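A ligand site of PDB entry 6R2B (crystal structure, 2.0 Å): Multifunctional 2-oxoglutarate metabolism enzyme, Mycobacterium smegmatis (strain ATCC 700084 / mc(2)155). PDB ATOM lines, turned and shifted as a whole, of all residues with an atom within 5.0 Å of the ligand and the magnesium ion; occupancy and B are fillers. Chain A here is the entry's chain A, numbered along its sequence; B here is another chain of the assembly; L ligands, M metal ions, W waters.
The magnesium ion is bound by the side-chain carboxylate of Asp 286 (1.9 Å), the side-chain amide oxygen of Asn 319 (2.0 Å), the backbone carbonyl oxygen of Ile 321 (2.1 Å), an oxygen (O2) of the ligand (2.2 Å), an oxygen (O6) of the ligand (2.2 Å) and water W4 (2.2 Å).
The nearest printed residue that does not touch the magnesium ion is Gly 322 (4.2 Å).
Water W6 bridges O13 of the ligand and ND1 of His 180.
Water W1 lies within hydrogen-bond range of a ring nitrogen (ND1) of His 388 (2.8 Å), the backbone NH (N) of Phe 323 (2.9 Å) and an oxygen (O5) of the ligand (2.9 Å).
Water W8 bridges O10 of the ligand and NZ of Lys 145.
Water W9 lies within hydrogen-bond range of the side-chain hydroxyl of Tyr 219, the side-chain amino group of Lys 145, an oxygen (O8) of the ligand and a ring nitrogen (NE2) of His 661 of chain B.
Water W2 bridges the backbone carbonyl oxygen of Phe 621 of chain B and the side-chain carboxylate of Glu 593 of chain B.
Water W5 bridges the side-chain carboxylate (OD2) of Asp 543 of chain B (2.7 Å) and the backbone carbonyl oxygen (O) of Gly 322 (3.0 Å).
The backbone NH (N) of Ala 287 sits close to an oxygen (O2) of the ligand, at 3.1 Å.
The side-chain hydroxyl (OG) of Ser 245 lies within hydrogen-bond range of an oxygen (O12) of the ligand (2.7 Å).
An oxygen (O9) of the ligand sits close to the side-chain amide oxygen of Gln 617 of chain B, at 2.6 Å.
A nitrogen (N2) of the ligand is in hydrogen-bond range of the backbone NH (N) of Leu 247 (3.0 Å).
An oxygen (O5) of the ligand is in hydrogen-bond range of a ring nitrogen (NE2) of His 180 (2.8 Å).
NH2 of Arg 181 lies within salt-bridge range of O5 of the ligand, at 2.9 Å.
O3 of the ligand lies within hydrogen-bond range of N of Ala 288 (3.1 Å).
The side-chain carboxylate (OE1) of Glu 593 of chain B is in hydrogen-bond range of a nitrogen (N1) of the ligand (2.6 Å).
NZ of Lys 145 lies within salt-bridge range of O8 of the ligand (3.8 Å).
O8 of the ligand lies within hydrogen-bond range of NE2 of His 661 of chain B (2.7 Å).
The backbone carbonyl oxygen of Ser 245 sits at hydrogen-bond distance from a nitrogen (N3) of the ligand (2.7 Å).
An oxygen (O13) of the ligand is in hydrogen-bond range of a ring nitrogen (NE2) of His 220 (2.9 Å).
A ring nitrogen (NE2) of His 388 sits at hydrogen-bond distance from an oxygen (O10) of the ligand (2.8 Å).
NE2 of His 220 sits close to OG of Ser 245.
OD2 of Asp 543 of chain B lies within hydrogen-bond range of NE2 of Gln 617 of chain B.
O of Gln 542 of chain B sits at hydrogen-bond distance from NE2 of Gln 617 of chain B.
The guanidinium group (NH2) of Arg 181 is in hydrogen-bond range of the backbone carbonyl oxygen (O) of His 388 (2.8 Å).
NE2 of Gln 292 sits at hydrogen-bond distance from O of Leu 591 of chain B (3.0 Å).
NE2 of Gln 542 of chain B lies within hydrogen-bond range of OE1 of Glu 593 of chain B, 2.9 Å away.
OE2 of Glu 593 of chain B is in hydrogen-bond range of NE2 of Gln 292 (3.0 Å).
CZ of Phe 147 touches C14 of the ligand, 3.7 Å away.
CE1 of Tyr 219 touches O13 of the ligand (3.6 Å).
His 246 touches the ligand (CA to N2, 3.5 Å).
Gly 285 touches the ligand.
Gln 292 touches the ligand.
Gly 322 touches the ligand.
OE1 of Gln 542 of chain B touches C5 of the ligand, 3.0 Å away.
Leu 591 of chain B touches the ligand (CD2 to N1, 3.6 Å).
CE1 of Phe 618 of chain B touches O9 of the ligand, 3.5 Å away.
Phe 621 of chain B touches the ligand (CE1 to C3, 3.5 Å).
Hydrophobic or aromatic side chains within 4 Å of the ligand: Phe 147, His 180, Tyr 219, His 220, Leu 247, Ala 287, Ala 288, His 388, Leu 591 of chain B, Phe 618 of chain B, Phe 621 of chain B and His 661 of chain B.
The nearest printed residue that does not touch the ligand is Phe 323 (4.02 Å).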
ATOM      1  N   LYS A 145      32.869  -1.853  -0.495  1.00  0.00           N
ATOM      2  CA  LYS A 145      31.735  -2.784  -0.619  1.00  0.00           C
ATOM      3  C   LYS A 145      30.499  -2.117  -1.170  1.00  0.00           C
ATOM      4  O   LYS A 145      29.991  -1.158  -0.579  1.00  0.00           O
ATOM      5  CB  LYS A 145      31.398  -3.429   0.726  1.00  0.00           C
ATOM      6  CG  LYS A 145      31.929  -4.843   0.891  1.00  0.00           C
ATOM      7  CD  LYS A 145      31.424  -5.485   2.174  1.00  0.00           C
ATOM      8  CE  LYS A 145      32.455  -6.431   2.697  1.00  0.00           C
ATOM      9  NZ  LYS A 145      31.884  -7.380   3.699  1.00  0.00           N
ATOM     10  N   PHE A 147      28.425  -4.577  -3.444  1.00  0.00           N
ATOM     11  CA  PHE A 147      27.777  -5.798  -3.956  1.00  0.00           C
ATOM     12  C   PHE A 147      27.078  -5.514  -5.275  1.00  0.00           C
ATOM     13  O   PHE A 147      25.847  -5.653  -5.407  1.00  0.00           O
ATOM     14  CB  PHE A 147      26.804  -6.432  -2.950  1.00  0.00           C
ATOM     15  CG  PHE A 147      27.487  -7.013  -1.748  1.00  0.00           C
ATOM     16  CD1 PHE A 147      28.255  -8.170  -1.844  1.00  0.00           C
ATOM     17  CD2 PHE A 147      27.344  -6.410  -0.486  1.00  0.00           C
ATOM     18  CE1 PHE A 147      28.888  -8.706  -0.724  1.00  0.00           C
ATOM     19  CE2 PHE A 147      28.005  -6.942   0.636  1.00  0.00           C
ATOM     20  CZ  PHE A 147      28.752  -8.095   0.518  1.00  0.00           C
ATOM     21  N   HIS A 180      21.416  -8.200  -0.723  1.00  0.00           N
ATOM     22  CA  HIS A 180      22.499  -7.268  -1.071  1.00  0.00           C
ATOM     23  C   HIS A 180      22.796  -7.103  -2.575  1.00  0.00           C
ATOM     24  O   HIS A 180      23.221  -6.031  -2.960  1.00  0.00           O
ATOM     25  CB  HIS A 180      23.788  -7.747  -0.391  1.00  0.00           C
ATOM     26  CG  HIS A 180      24.121  -9.177  -0.699  1.00  0.00           C
ATOM     27  ND1 HIS A 180      23.379 -10.223  -0.171  1.00  0.00           N
ATOM     28  CD2 HIS A 180      25.072  -9.701  -1.516  1.00  0.00           C
ATOM     29  CE1 HIS A 180      23.910 -11.332  -0.647  1.00  0.00           C
ATOM     30  NE2 HIS A 180      24.923 -11.082  -1.462  1.00  0.00           N
ATOM     31  N   ARG A 181      22.649  -8.162  -3.397  1.00  0.00           N
ATOM     32  CA  ARG A 181      23.026  -8.131  -4.824  1.00  0.00           C
ATOM     33  C   ARG A 181      22.243  -7.084  -5.623  1.00  0.00           C
ATOM     34  O   ARG A 181      21.080  -7.263  -5.899  1.00  0.00           O
ATOM     35  CB  ARG A 181      22.848  -9.544  -5.452  1.00  0.00           C
ATOM     36  CG  ARG A 181      23.596  -9.805  -6.791  1.00  0.00           C
ATOM     37  CD  ARG A 181      25.085  -9.479  -6.757  1.00  0.00           C
ATOM     38  NE  ARG A 181      25.819 -10.275  -5.761  1.00  0.00           N
ATOM     39  CZ  ARG A 181      27.080 -10.066  -5.403  1.00  0.00           C
ATOM     40  NH1 ARG A 181      27.770  -9.061  -5.933  1.00  0.00           N
ATOM     41  NH2 ARG A 181      27.665 -10.868  -4.518  1.00  0.00           N
ATOM     42  N   TYR A 219      23.570  -1.227   2.099  1.00  0.00           N
ATOM     43  CA  TYR A 219      22.897  -2.243   1.302  1.00  0.00           C
ATOM     44  C   TYR A 219      21.786  -2.958   2.115  1.00  0.00           C
ATOM     45  O   TYR A 219      21.258  -3.980   1.683  1.00  0.00           O
ATOM     46  CB  TYR A 219      23.896  -3.247   0.676  1.00  0.00           C
ATOM     47  CG  TYR A 219      25.019  -3.692   1.580  1.00  0.00           C
ATOM     48  CD1 TYR A 219      24.841  -4.753   2.475  1.00  0.00           C
ATOM     49  CD2 TYR A 219      26.289  -3.113   1.498  1.00  0.00           C
ATOM     50  CE1 TYR A 219      25.888  -5.212   3.265  1.00  0.00           C
ATOM     51  CE2 TYR A 219      27.331  -3.549   2.313  1.00  0.00           C
ATOM     52  CZ  TYR A 219      27.120  -4.582   3.203  1.00  0.00           C
ATOM     53  OH  TYR A 219      28.140  -5.010   4.013  1.00  0.00           O
ATOM     54  N   HIS A 220      21.359  -2.358   3.243  1.00  0.00           N
ATOM     55  CA  HIS A 220      20.247  -2.887   4.054  1.00  0.00           C
ATOM     56  C   HIS A 220      19.108  -1.919   4.146  1.00  0.00           C
ATOM     57  O   HIS A 220      18.102  -2.215   4.776  1.00  0.00           O
ATOM     58  CB  HIS A 220      20.724  -3.182   5.486  1.00  0.00           C
ATOM     59  CG  HIS A 220      21.553  -4.425   5.608  1.00  0.00           C
ATOM     60  ND1 HIS A 220      22.069  -4.810   6.816  1.00  0.00           N
ATOM     61  CD2 HIS A 220      21.951  -5.283   4.652  1.00  0.00           C
ATOM     62  CE1 HIS A 220      22.779  -5.896   6.565  1.00  0.00           C
ATOM     63  NE2 HIS A 220      22.757  -6.211   5.270  1.00  0.00           N
ATOM     64  N   PRO A 244      18.139  -7.274   7.686  1.00  0.00           N
ATOM     65  CA  PRO A 244      19.470  -7.508   8.235  1.00  0.00           C
ATOM     66  C   PRO A 244      20.317  -8.262   7.204  1.00  0.00           C
ATOM     67  O   PRO A 244      19.825  -8.571   6.110  1.00  0.00           O
ATOM     68  CB  PRO A 244      19.181  -8.355   9.478  1.00  0.00           C
ATOM     69  CG  PRO A 244      17.957  -9.176   9.085  1.00  0.00           C
ATOM     70  CD  PRO A 244      17.192  -8.356   8.068  1.00  0.00           C
ATOM     71  N   SER A 245      21.557  -8.609   7.578  1.00  0.00           N
ATOM     72  CA  SER A 245      22.445  -9.388   6.713  1.00  0.00           C
ATOM     73  C   SER A 245      21.882 -10.792   6.517  1.00  0.00           C
ATOM     74  O   SER A 245      22.054 -11.355   5.446  1.00  0.00           O
ATOM     75  CB  SER A 245      23.847  -9.449   7.300  1.00  0.00           C
ATOM     76  OG  SER A 245      24.609  -8.262   7.147  1.00  0.00           O
ATOM     77  N   HIS A 246      21.180 -11.335   7.533  1.00  0.00           N
ATOM     78  CA  HIS A 246      20.572 -12.698   7.542  1.00  0.00           C
ATOM     79  C   HIS A 246      19.707 -12.894   6.313  1.00  0.00           C
ATOM     80  O   HIS A 246      18.612 -12.326   6.196  1.00  0.00           O
ATOM     81  CB  HIS A 246      19.790 -12.920   8.843  1.00  0.00           C
ATOM     82  CG  HIS A 246      20.676 -12.889  10.060  1.00  0.00           C
ATOM     83  ND1 HIS A 246      21.452 -11.778  10.356  1.00  0.00           N
ATOM     84  CD2 HIS A 246      20.886 -13.838  10.997  1.00  0.00           C
ATOM     85  CE1 HIS A 246      22.115 -12.096  11.463  1.00  0.00           C
ATOM     86  NE2 HIS A 246      21.804 -13.315  11.891  1.00  0.00           N
ATOM     87  N   LEU A 247      20.269 -13.606   5.341  1.00  0.00           N
ATOM     88  CA  LEU A 247      19.650 -13.825   4.038  1.00  0.00           C
ATOM     89  C   LEU A 247      18.376 -14.604   4.209  1.00  0.00           C
ATOM     90  O   LEU A 247      18.335 -15.566   4.977  1.00  0.00           O
ATOM     91  CB  LEU A 247      20.612 -14.524   3.061  1.00  0.00           C
ATOM     92  CG  LEU A 247      21.990 -13.818   2.818  1.00  0.00           C
ATOM     93  CD1 LEU A 247      22.973 -14.724   2.101  1.00  0.00           C
ATOM     94  CD2 LEU A 247      21.838 -12.557   2.059  1.00  0.00           C
ATOM     95  N   GLY A 285      19.058 -14.608  -3.666  1.00  0.00           N
ATOM     96  CA  GLY A 285      20.316 -15.058  -4.245  1.00  0.00           C
ATOM     97  C   GLY A 285      20.175 -16.565  -4.392  1.00  0.00           C
ATOM     98  O   GLY A 285      19.389 -17.166  -3.658  1.00  0.00           O
ATOM     99  N   ASP A 286      20.907 -17.193  -5.329  1.00  0.00           N
ATOM    100  CA  ASP A 286      20.794 -18.635  -5.602  1.00  0.00           C
ATOM    101  C   ASP A 286      21.208 -19.543  -4.419  1.00  0.00           C
ATOM    102  O   ASP A 286      20.531 -20.534  -4.195  1.00  0.00           O
ATOM    103  CB  ASP A 286      21.561 -19.042  -6.892  1.00  0.00           C
ATOM    104  CG  ASP A 286      23.053 -18.649  -6.946  1.00  0.00           C
ATOM    105  OD1 ASP A 286      23.347 -17.461  -6.801  1.00  0.00           O
ATOM    106  OD2 ASP A 286      23.899 -19.543  -7.203  1.00  0.00           O
ATOM    107  N   ALA A 287      22.348 -19.271  -3.749  1.00  0.00           N
ATOM    108  CA  ALA A 287      22.783 -20.173  -2.655  1.00  0.00           C
ATOM    109  C   ALA A 287      21.857 -20.036  -1.450  1.00  0.00           C
ATOM    110  O   ALA A 287      21.495 -21.050  -0.874  1.00  0.00           O
ATOM    111  CB  ALA A 287      24.231 -19.901  -2.255  1.00  0.00           C
ATOM    112  N   ALA A 288      21.404 -18.795  -1.135  1.00  0.00           N
ATOM    113  CA  ALA A 288      20.513 -18.569  -0.001  1.00  0.00           C
ATOM    114  C   ALA A 288      19.111 -19.176  -0.220  1.00  0.00           C
ATOM    115  O   ALA A 288      18.544 -19.723   0.735  1.00  0.00           O
ATOM    116  CB  ALA A 288      20.395 -17.077   0.281  1.00  0.00           C
ATOM    117  N   GLN A 292      18.424 -21.767   2.945  1.00  0.00           N
ATOM    118  CA  GLN A 292      17.733 -21.209   4.136  1.00  0.00           C
ATOM    119  C   GLN A 292      16.286 -21.755   4.297  1.00  0.00           C
ATOM    120  O   GLN A 292      15.443 -21.557   3.437  1.00  0.00           O
ATOM    121  CB  GLN A 292      17.727 -19.672   4.080  1.00  0.00           C
ATOM    122  CG  GLN A 292      19.121 -19.069   4.306  1.00  0.00           C
ATOM    123  CD  GLN A 292      19.555 -19.155   5.768  1.00  0.00           C
ATOM    124  OE1 GLN A 292      18.867 -18.711   6.694  1.00  0.00           O
ATOM    125  NE2 GLN A 292      20.715 -19.735   6.003  1.00  0.00           N
ATOM    126  N   VAL A 317      18.247 -13.972  -8.389  1.00  0.00           N
ATOM    127  CA  VAL A 317      19.400 -13.457  -9.144  1.00  0.00           C
ATOM    128  C   VAL A 317      20.401 -14.609  -9.113  1.00  0.00           C
ATOM    129  O   VAL A 317      21.219 -14.724  -8.198  1.00  0.00           O
ATOM    130  CB  VAL A 317      19.974 -12.128  -8.552  1.00  0.00           C
ATOM    131  CG1 VAL A 317      21.118 -11.598  -9.407  1.00  0.00           C
ATOM    132  CG2 VAL A 317      18.886 -11.073  -8.379  1.00  0.00           C
ATOM    133  N   ASN A 319      23.365 -15.991 -10.128  1.00  0.00           N
ATOM    134  CA  ASN A 319      24.703 -15.728 -10.706  1.00  0.00           C
ATOM    135  C   ASN A 319      25.613 -16.979 -10.579  1.00  0.00           C
ATOM    136  O   ASN A 319      26.813 -16.890 -10.779  1.00  0.00           O
ATOM    137  CB  ASN A 319      25.353 -14.497 -10.053  1.00  0.00           C
ATOM    138  CG  ASN A 319      25.230 -14.481  -8.566  1.00  0.00           C
ATOM    139  OD1 ASN A 319      25.102 -15.509  -7.924  1.00  0.00           O
ATOM    140  ND2 ASN A 319      25.219 -13.302  -7.988  1.00  0.00           N
ATOM    141  N   GLN A 320      25.006 -18.125 -10.286  1.00  0.00           N
ATOM    142  CA  GLN A 320      25.603 -19.474 -10.285  1.00  0.00           C
ATOM    143  C   GLN A 320      26.852 -19.590  -9.379  1.00  0.00           C
ATOM    144  O   GLN A 320      27.774 -20.353  -9.683  1.00  0.00           O
ATOM    145  CB  GLN A 320      25.918 -19.889 -11.744  1.00  0.00           C
ATOM    146  CG  GLN A 320      24.723 -19.689 -12.699  1.00  0.00           C
ATOM    147  CD  GLN A 320      25.080 -19.971 -14.144  1.00  0.00           C
ATOM    148  OE1 GLN A 320      25.362 -21.099 -14.524  1.00  0.00           O
ATOM    149  NE2 GLN A 320      25.106 -18.935 -14.966  1.00  0.00           N
ATOM    150  N   ILE A 321      26.839 -18.874  -8.261  1.00  0.00           N
ATOM    151  CA  ILE A 321      27.882 -18.842  -7.224  1.00  0.00           C
ATOM    152  C   ILE A 321      27.307 -18.238  -5.952  1.00  0.00           C
ATOM    153  O   ILE A 321      26.419 -17.380  -6.014  1.00  0.00           O
ATOM    154  CB  ILE A 321      29.134 -18.028  -7.746  1.00  0.00           C
ATOM    155  CG1 ILE A 321      30.355 -18.154  -6.829  1.00  0.00           C
ATOM    156  CG2 ILE A 321      28.814 -16.529  -8.026  1.00  0.00           C
ATOM    157  CD1 ILE A 321      31.101 -19.328  -6.978  1.00  0.00           C
ATOM    158  N   GLY A 322      27.864 -18.677  -4.811  1.00  0.00           N
ATOM    159  CA  GLY A 322      27.571 -18.149  -3.489  1.00  0.00           C
ATOM    160  C   GLY A 322      28.916 -17.836  -2.854  1.00  0.00           C
ATOM    161  O   GLY A 322      29.539 -18.723  -2.291  1.00  0.00           O
ATOM    162  N   PHE A 323      29.418 -16.598  -3.013  1.00  0.00           N
ATOM    163  CA  PHE A 323      30.734 -16.179  -2.496  1.00  0.00           C
ATOM    164  C   PHE A 323      31.828 -16.981  -3.201  1.00  0.00           C
ATOM    165  O   PHE A 323      32.096 -16.701  -4.371  1.00  0.00           O
ATOM    166  CB  PHE A 323      30.809 -16.311  -0.951  1.00  0.00           C
ATOM    167  CG  PHE A 323      31.864 -15.484  -0.239  1.00  0.00           C
ATOM    168  CD1 PHE A 323      32.991 -15.022  -0.924  1.00  0.00           C
ATOM    169  CD2 PHE A 323      31.740 -15.175   1.112  1.00  0.00           C
ATOM    170  CE1 PHE A 323      33.936 -14.232  -0.281  1.00  0.00           C
ATOM    171  CE2 PHE A 323      32.700 -14.392   1.753  1.00  0.00           C
ATOM    172  CZ  PHE A 323      33.794 -13.943   1.055  1.00  0.00           C
ATOM    173  N   HIS A 388      32.847 -11.636  -5.019  1.00  0.00           N
ATOM    174  CA  HIS A 388      31.646 -11.632  -4.166  1.00  0.00           C
ATOM    175  C   HIS A 388      31.319 -10.214  -3.711  1.00  0.00           C
ATOM    176  O   HIS A 388      30.160  -9.771  -3.764  1.00  0.00           O
ATOM    177  CB  HIS A 388      31.874 -12.511  -2.952  1.00  0.00           C
ATOM    178  CG  HIS A 388      30.719 -12.518  -2.020  1.00  0.00           C
ATOM    179  ND1 HIS A 388      29.449 -12.853  -2.450  1.00  0.00           N
ATOM    180  CD2 HIS A 388      30.681 -12.280  -0.695  1.00  0.00           C
ATOM    181  CE1 HIS A 388      28.693 -12.773  -1.379  1.00  0.00           C
ATOM    182  NE2 HIS A 388      29.403 -12.471  -0.301  1.00  0.00           N
ATOM    183  N   GLN B 542      30.674 -21.982   5.865  1.00  0.00           N
ATOM    184  CA  GLN B 542      30.503 -21.154   4.669  1.00  0.00           C
ATOM    185  C   GLN B 542      31.829 -20.590   4.179  1.00  0.00           C
ATOM    186  O   GLN B 542      32.497 -19.818   4.902  1.00  0.00           O
ATOM    187  CB  GLN B 542      29.472 -20.044   4.925  1.00  0.00           C
ATOM    188  CG  GLN B 542      28.028 -20.572   4.820  1.00  0.00           C
ATOM    189  CD  GLN B 542      27.055 -19.792   5.669  1.00  0.00           C
ATOM    190  OE1 GLN B 542      27.212 -18.601   5.905  1.00  0.00           O
ATOM    191  NE2 GLN B 542      26.004 -20.450   6.141  1.00  0.00           N
ATOM    192  N   ASP B 543      32.240 -21.057   2.982  1.00  0.00           N
ATOM    193  CA  ASP B 543      33.488 -20.705   2.271  1.00  0.00           C
ATOM    194  C   ASP B 543      34.728 -21.053   3.123  1.00  0.00           C
ATOM    195  O   ASP B 543      35.748 -20.387   3.034  1.00  0.00           O
ATOM    196  CB  ASP B 543      33.428 -19.215   1.891  1.00  0.00           C
ATOM    197  CG  ASP B 543      32.146 -18.919   1.125  1.00  0.00           C
ATOM    198  OD1 ASP B 543      32.038 -19.345  -0.040  1.00  0.00           O
ATOM    199  OD2 ASP B 543      31.226 -18.303   1.720  1.00  0.00           O
ATOM    200  N   LEU B 591      24.471 -22.936   2.299  1.00  0.00           N
ATOM    201  CA  LEU B 591      24.224 -21.695   3.020  1.00  0.00           C
ATOM    202  C   LEU B 591      23.114 -21.936   4.043  1.00  0.00           C
ATOM    203  O   LEU B 591      21.965 -21.502   3.879  1.00  0.00           O
ATOM    204  CB  LEU B 591      23.868 -20.550   2.068  1.00  0.00           C
ATOM    205  CG  LEU B 591      24.407 -19.163   2.439  1.00  0.00           C
ATOM    206  CD1 LEU B 591      24.345 -18.253   1.253  1.00  0.00           C
ATOM    207  CD2 LEU B 591      23.649 -18.535   3.611  1.00  0.00           C
ATOM    208  N   GLU B 593      22.649 -22.628   8.567  1.00  0.00           N
ATOM    209  CA  GLU B 593      23.217 -22.558   9.918  1.00  0.00           C
ATOM    210  C   GLU B 593      22.547 -23.648  10.733  1.00  0.00           C
ATOM    211  O   GLU B 593      23.234 -24.542  11.234  1.00  0.00           O
ATOM    212  CB  GLU B 593      23.065 -21.161  10.565  1.00  0.00           C
ATOM    213  CG  GLU B 593      24.040 -20.099  10.054  1.00  0.00           C
ATOM    214  CD  GLU B 593      23.645 -19.433   8.745  1.00  0.00           C
ATOM    215  OE1 GLU B 593      24.545 -18.858   8.079  1.00  0.00           O
ATOM    216  OE2 GLU B 593      22.455 -19.494   8.378  1.00  0.00           O
ATOM    217  N   GLN B 617      30.308 -17.915   9.059  1.00  0.00           N
ATOM    218  CA  GLN B 617      30.947 -16.951   8.162  1.00  0.00           C
ATOM    219  C   GLN B 617      31.399 -15.758   9.041  1.00  0.00           C
ATOM    220  O   GLN B 617      32.559 -15.313   8.996  1.00  0.00           O
ATOM    221  CB  GLN B 617      29.996 -16.527   7.033  1.00  0.00           C
ATOM    222  CG  GLN B 617      30.689 -15.529   6.104  1.00  0.00           C
ATOM    223  CD  GLN B 617      30.595 -15.907   4.655  1.00  0.00           C
ATOM    224  OE1 GLN B 617      29.930 -15.243   3.889  1.00  0.00           O
ATOM    225  NE2 GLN B 617      31.294 -16.933   4.245  1.00  0.00           N
ATOM    226  N   PHE B 618      30.458 -15.305   9.876  1.00  0.00           N
ATOM    227  CA  PHE B 618      30.589 -14.301  10.942  1.00  0.00           C
ATOM    228  C   PHE B 618      29.776 -14.842  12.094  1.00  0.00           C
ATOM    229  O   PHE B 618      28.696 -15.376  11.847  1.00  0.00           O
ATOM    230  CB  PHE B 618      30.091 -12.909  10.488  1.00  0.00           C
ATOM    231  CG  PHE B 618      30.990 -12.219   9.495  1.00  0.00           C
ATOM    232  CD1 PHE B 618      30.893 -12.487   8.127  1.00  0.00           C
ATOM    233  CD2 PHE B 618      31.951 -11.298   9.924  1.00  0.00           C
ATOM    234  CE1 PHE B 618      31.749 -11.874   7.201  1.00  0.00           C
ATOM    235  CE2 PHE B 618      32.781 -10.659   9.001  1.00  0.00           C
ATOM    236  CZ  PHE B 618      32.681 -10.954   7.645  1.00  0.00           C
ATOM    237  N   PHE B 621      25.758 -14.851  12.531  1.00  0.00           N
ATOM    238  CA  PHE B 621      24.769 -15.700  11.849  1.00  0.00           C
ATOM    239  C   PHE B 621      24.459 -16.996  12.612  1.00  0.00           C
ATOM    240  O   PHE B 621      23.507 -17.685  12.237  1.00  0.00           O
ATOM    241  CB  PHE B 621      25.230 -16.009  10.411  1.00  0.00           C
ATOM    242  CG  PHE B 621      25.436 -14.758   9.600  1.00  0.00           C
ATOM    243  CD1 PHE B 621      24.370 -13.896   9.332  1.00  0.00           C
ATOM    244  CD2 PHE B 621      26.706 -14.404   9.148  1.00  0.00           C
ATOM    245  CE1 PHE B 621      24.574 -12.697   8.652  1.00  0.00           C
ATOM    246  CE2 PHE B 621      26.912 -13.209   8.451  1.00  0.00           C
ATOM    247  CZ  PHE B 621      25.848 -12.367   8.206  1.00  0.00           C
ATOM    248  N   HIS B 661      28.092  -7.978  11.432  1.00  0.00           N
ATOM    249  CA  HIS B 661      29.479  -8.351  11.166  1.00  0.00           C
ATOM    250  C   HIS B 661      30.317  -7.911  12.346  1.00  0.00           C
ATOM    251  O   HIS B 661      31.421  -7.408  12.156  1.00  0.00           O
ATOM    252  CB  HIS B 661      29.993  -7.714   9.874  1.00  0.00           C
ATOM    253  CG  HIS B 661      29.325  -8.241   8.638  1.00  0.00           C
ATOM    254  ND1 HIS B 661      28.113  -7.738   8.213  1.00  0.00           N
ATOM    255  CD2 HIS B 661      29.719  -9.218   7.788  1.00  0.00           C
ATOM    256  CE1 HIS B 661      27.810  -8.413   7.114  1.00  0.00           C
ATOM    257  NE2 HIS B 661      28.727  -9.341   6.837  1.00  0.00           N
HETATM  258  N1  LIG L   1      24.171 -16.712   6.677  1.00  0.00           N
HETATM  259  C1  LIG L   1      23.097 -15.886   6.578  1.00  0.00           C
HETATM  260  C2  LIG L   1      21.781 -16.410   7.137  1.00  0.00           C
HETATM  261  N2  LIG L   1      23.041 -14.641   6.019  1.00  0.00           N
HETATM  262  C3  LIG L   1      24.255 -14.186   5.530  1.00  0.00           C
HETATM  263  N3  LIG L   1      24.241 -12.864   5.101  1.00  0.00           N
HETATM  264  C4  LIG L   1      25.472 -14.983   5.567  1.00  0.00           C
HETATM  265  C5  LIG L   1      25.369 -16.240   6.165  1.00  0.00           C
HETATM  266  C6  LIG L   1      26.784 -14.496   5.046  1.00  0.00           C
HETATM  267  N4  LIG L   1      26.802 -14.224   3.580  1.00  0.00           N
HETATM  268  C7  LIG L   1      26.501 -12.846   3.116  1.00  0.00           C
HETATM  269  S1  LIG L   1      26.366 -12.945   1.243  1.00  0.00           S
HETATM  270  C8  LIG L   1      26.708 -14.740   1.286  1.00  0.00           C
HETATM  271  C9  LIG L   1      26.883 -15.233   2.576  1.00  0.00           C
HETATM  272  C10 LIG L   1      27.169 -16.695   2.938  1.00  0.00           C
HETATM  273  C11 LIG L   1      26.720 -15.517   0.045  1.00  0.00           C
HETATM  274  C12 LIG L   1      25.356 -15.380  -0.718  1.00  0.00           C
HETATM  275  O1  LIG L   1      25.307 -16.104  -1.847  1.00  0.00           O
HETATM  276  P1  LIG L   1      23.978 -15.948  -2.920  1.00  0.00           P
HETATM  277  O2  LIG L   1      24.275 -16.889  -4.078  1.00  0.00           O
HETATM  278  O3  LIG L   1      22.814 -16.216  -2.076  1.00  0.00           O
HETATM  279  O4  LIG L   1      24.008 -14.437  -3.199  1.00  0.00           O
HETATM  280  P2  LIG L   1      25.062 -13.554  -4.190  1.00  0.00           P
HETATM  281  O5  LIG L   1      26.065 -12.906  -3.267  1.00  0.00           O
HETATM  282  O6  LIG L   1      25.732 -14.573  -5.077  1.00  0.00           O
HETATM  283  O7  LIG L   1      24.200 -12.508  -4.884  1.00  0.00           O
HETATM  284  C13 LIG L   1      27.253 -11.616   3.656  1.00  0.00           C
HETATM  285  P3  LIG L   1      29.203 -11.620   3.809  1.00  0.00           P
HETATM  286  O8  LIG L   1      29.514 -10.268   4.407  1.00  0.00           O
HETATM  287  O9  LIG L   1      29.454 -12.839   4.678  1.00  0.00           O
HETATM  288  O10 LIG L   1      29.687 -11.811   2.388  1.00  0.00           O
HETATM  289  C14 LIG L   1      26.919 -10.379   2.702  1.00  0.00           C
HETATM  290  O11 LIG L   1      26.726 -11.356   4.937  1.00  0.00           O
HETATM  291  C15 LIG L   1      25.489  -9.845   2.620  1.00  0.00           C
HETATM  292  C16 LIG L   1      25.049  -8.959   3.792  1.00  0.00           C
HETATM  293  O12 LIG L   1      25.740  -8.929   4.832  1.00  0.00           O
HETATM  294  O13 LIG L   1      24.023  -8.239   3.682  1.00  0.00           O
HETATM  295 MG    MG M   1      24.688 -16.252  -6.117  1.00  0.00          MG
HETATM  296  O   HOH W   1      28.319 -14.387  -4.460  1.00  0.00           O
HETATM  297  O   HOH W   2      21.545 -17.357  10.333  1.00  0.00           O
HETATM  298  O   HOH W   3      21.818 -11.979  -3.300  1.00  0.00           O
HETATM  299  O   HOH W   4      23.011 -14.772  -6.088  1.00  0.00           O
HETATM  300  O   HOH W   5      28.757 -18.683   0.626  1.00  0.00           O
HETATM  301  O   HOH W   6      22.022  -9.084   2.221  1.00  0.00           O
HETATM  302  O   HOH W   7      21.522 -13.963  -1.274  1.00  0.00           O
HETATM  303  O   HOH W   8      31.451  -9.786   1.833  1.00  0.00           O
HETATM  304  O   HOH W   9      29.184  -7.483   4.291  1.00  0.00           O
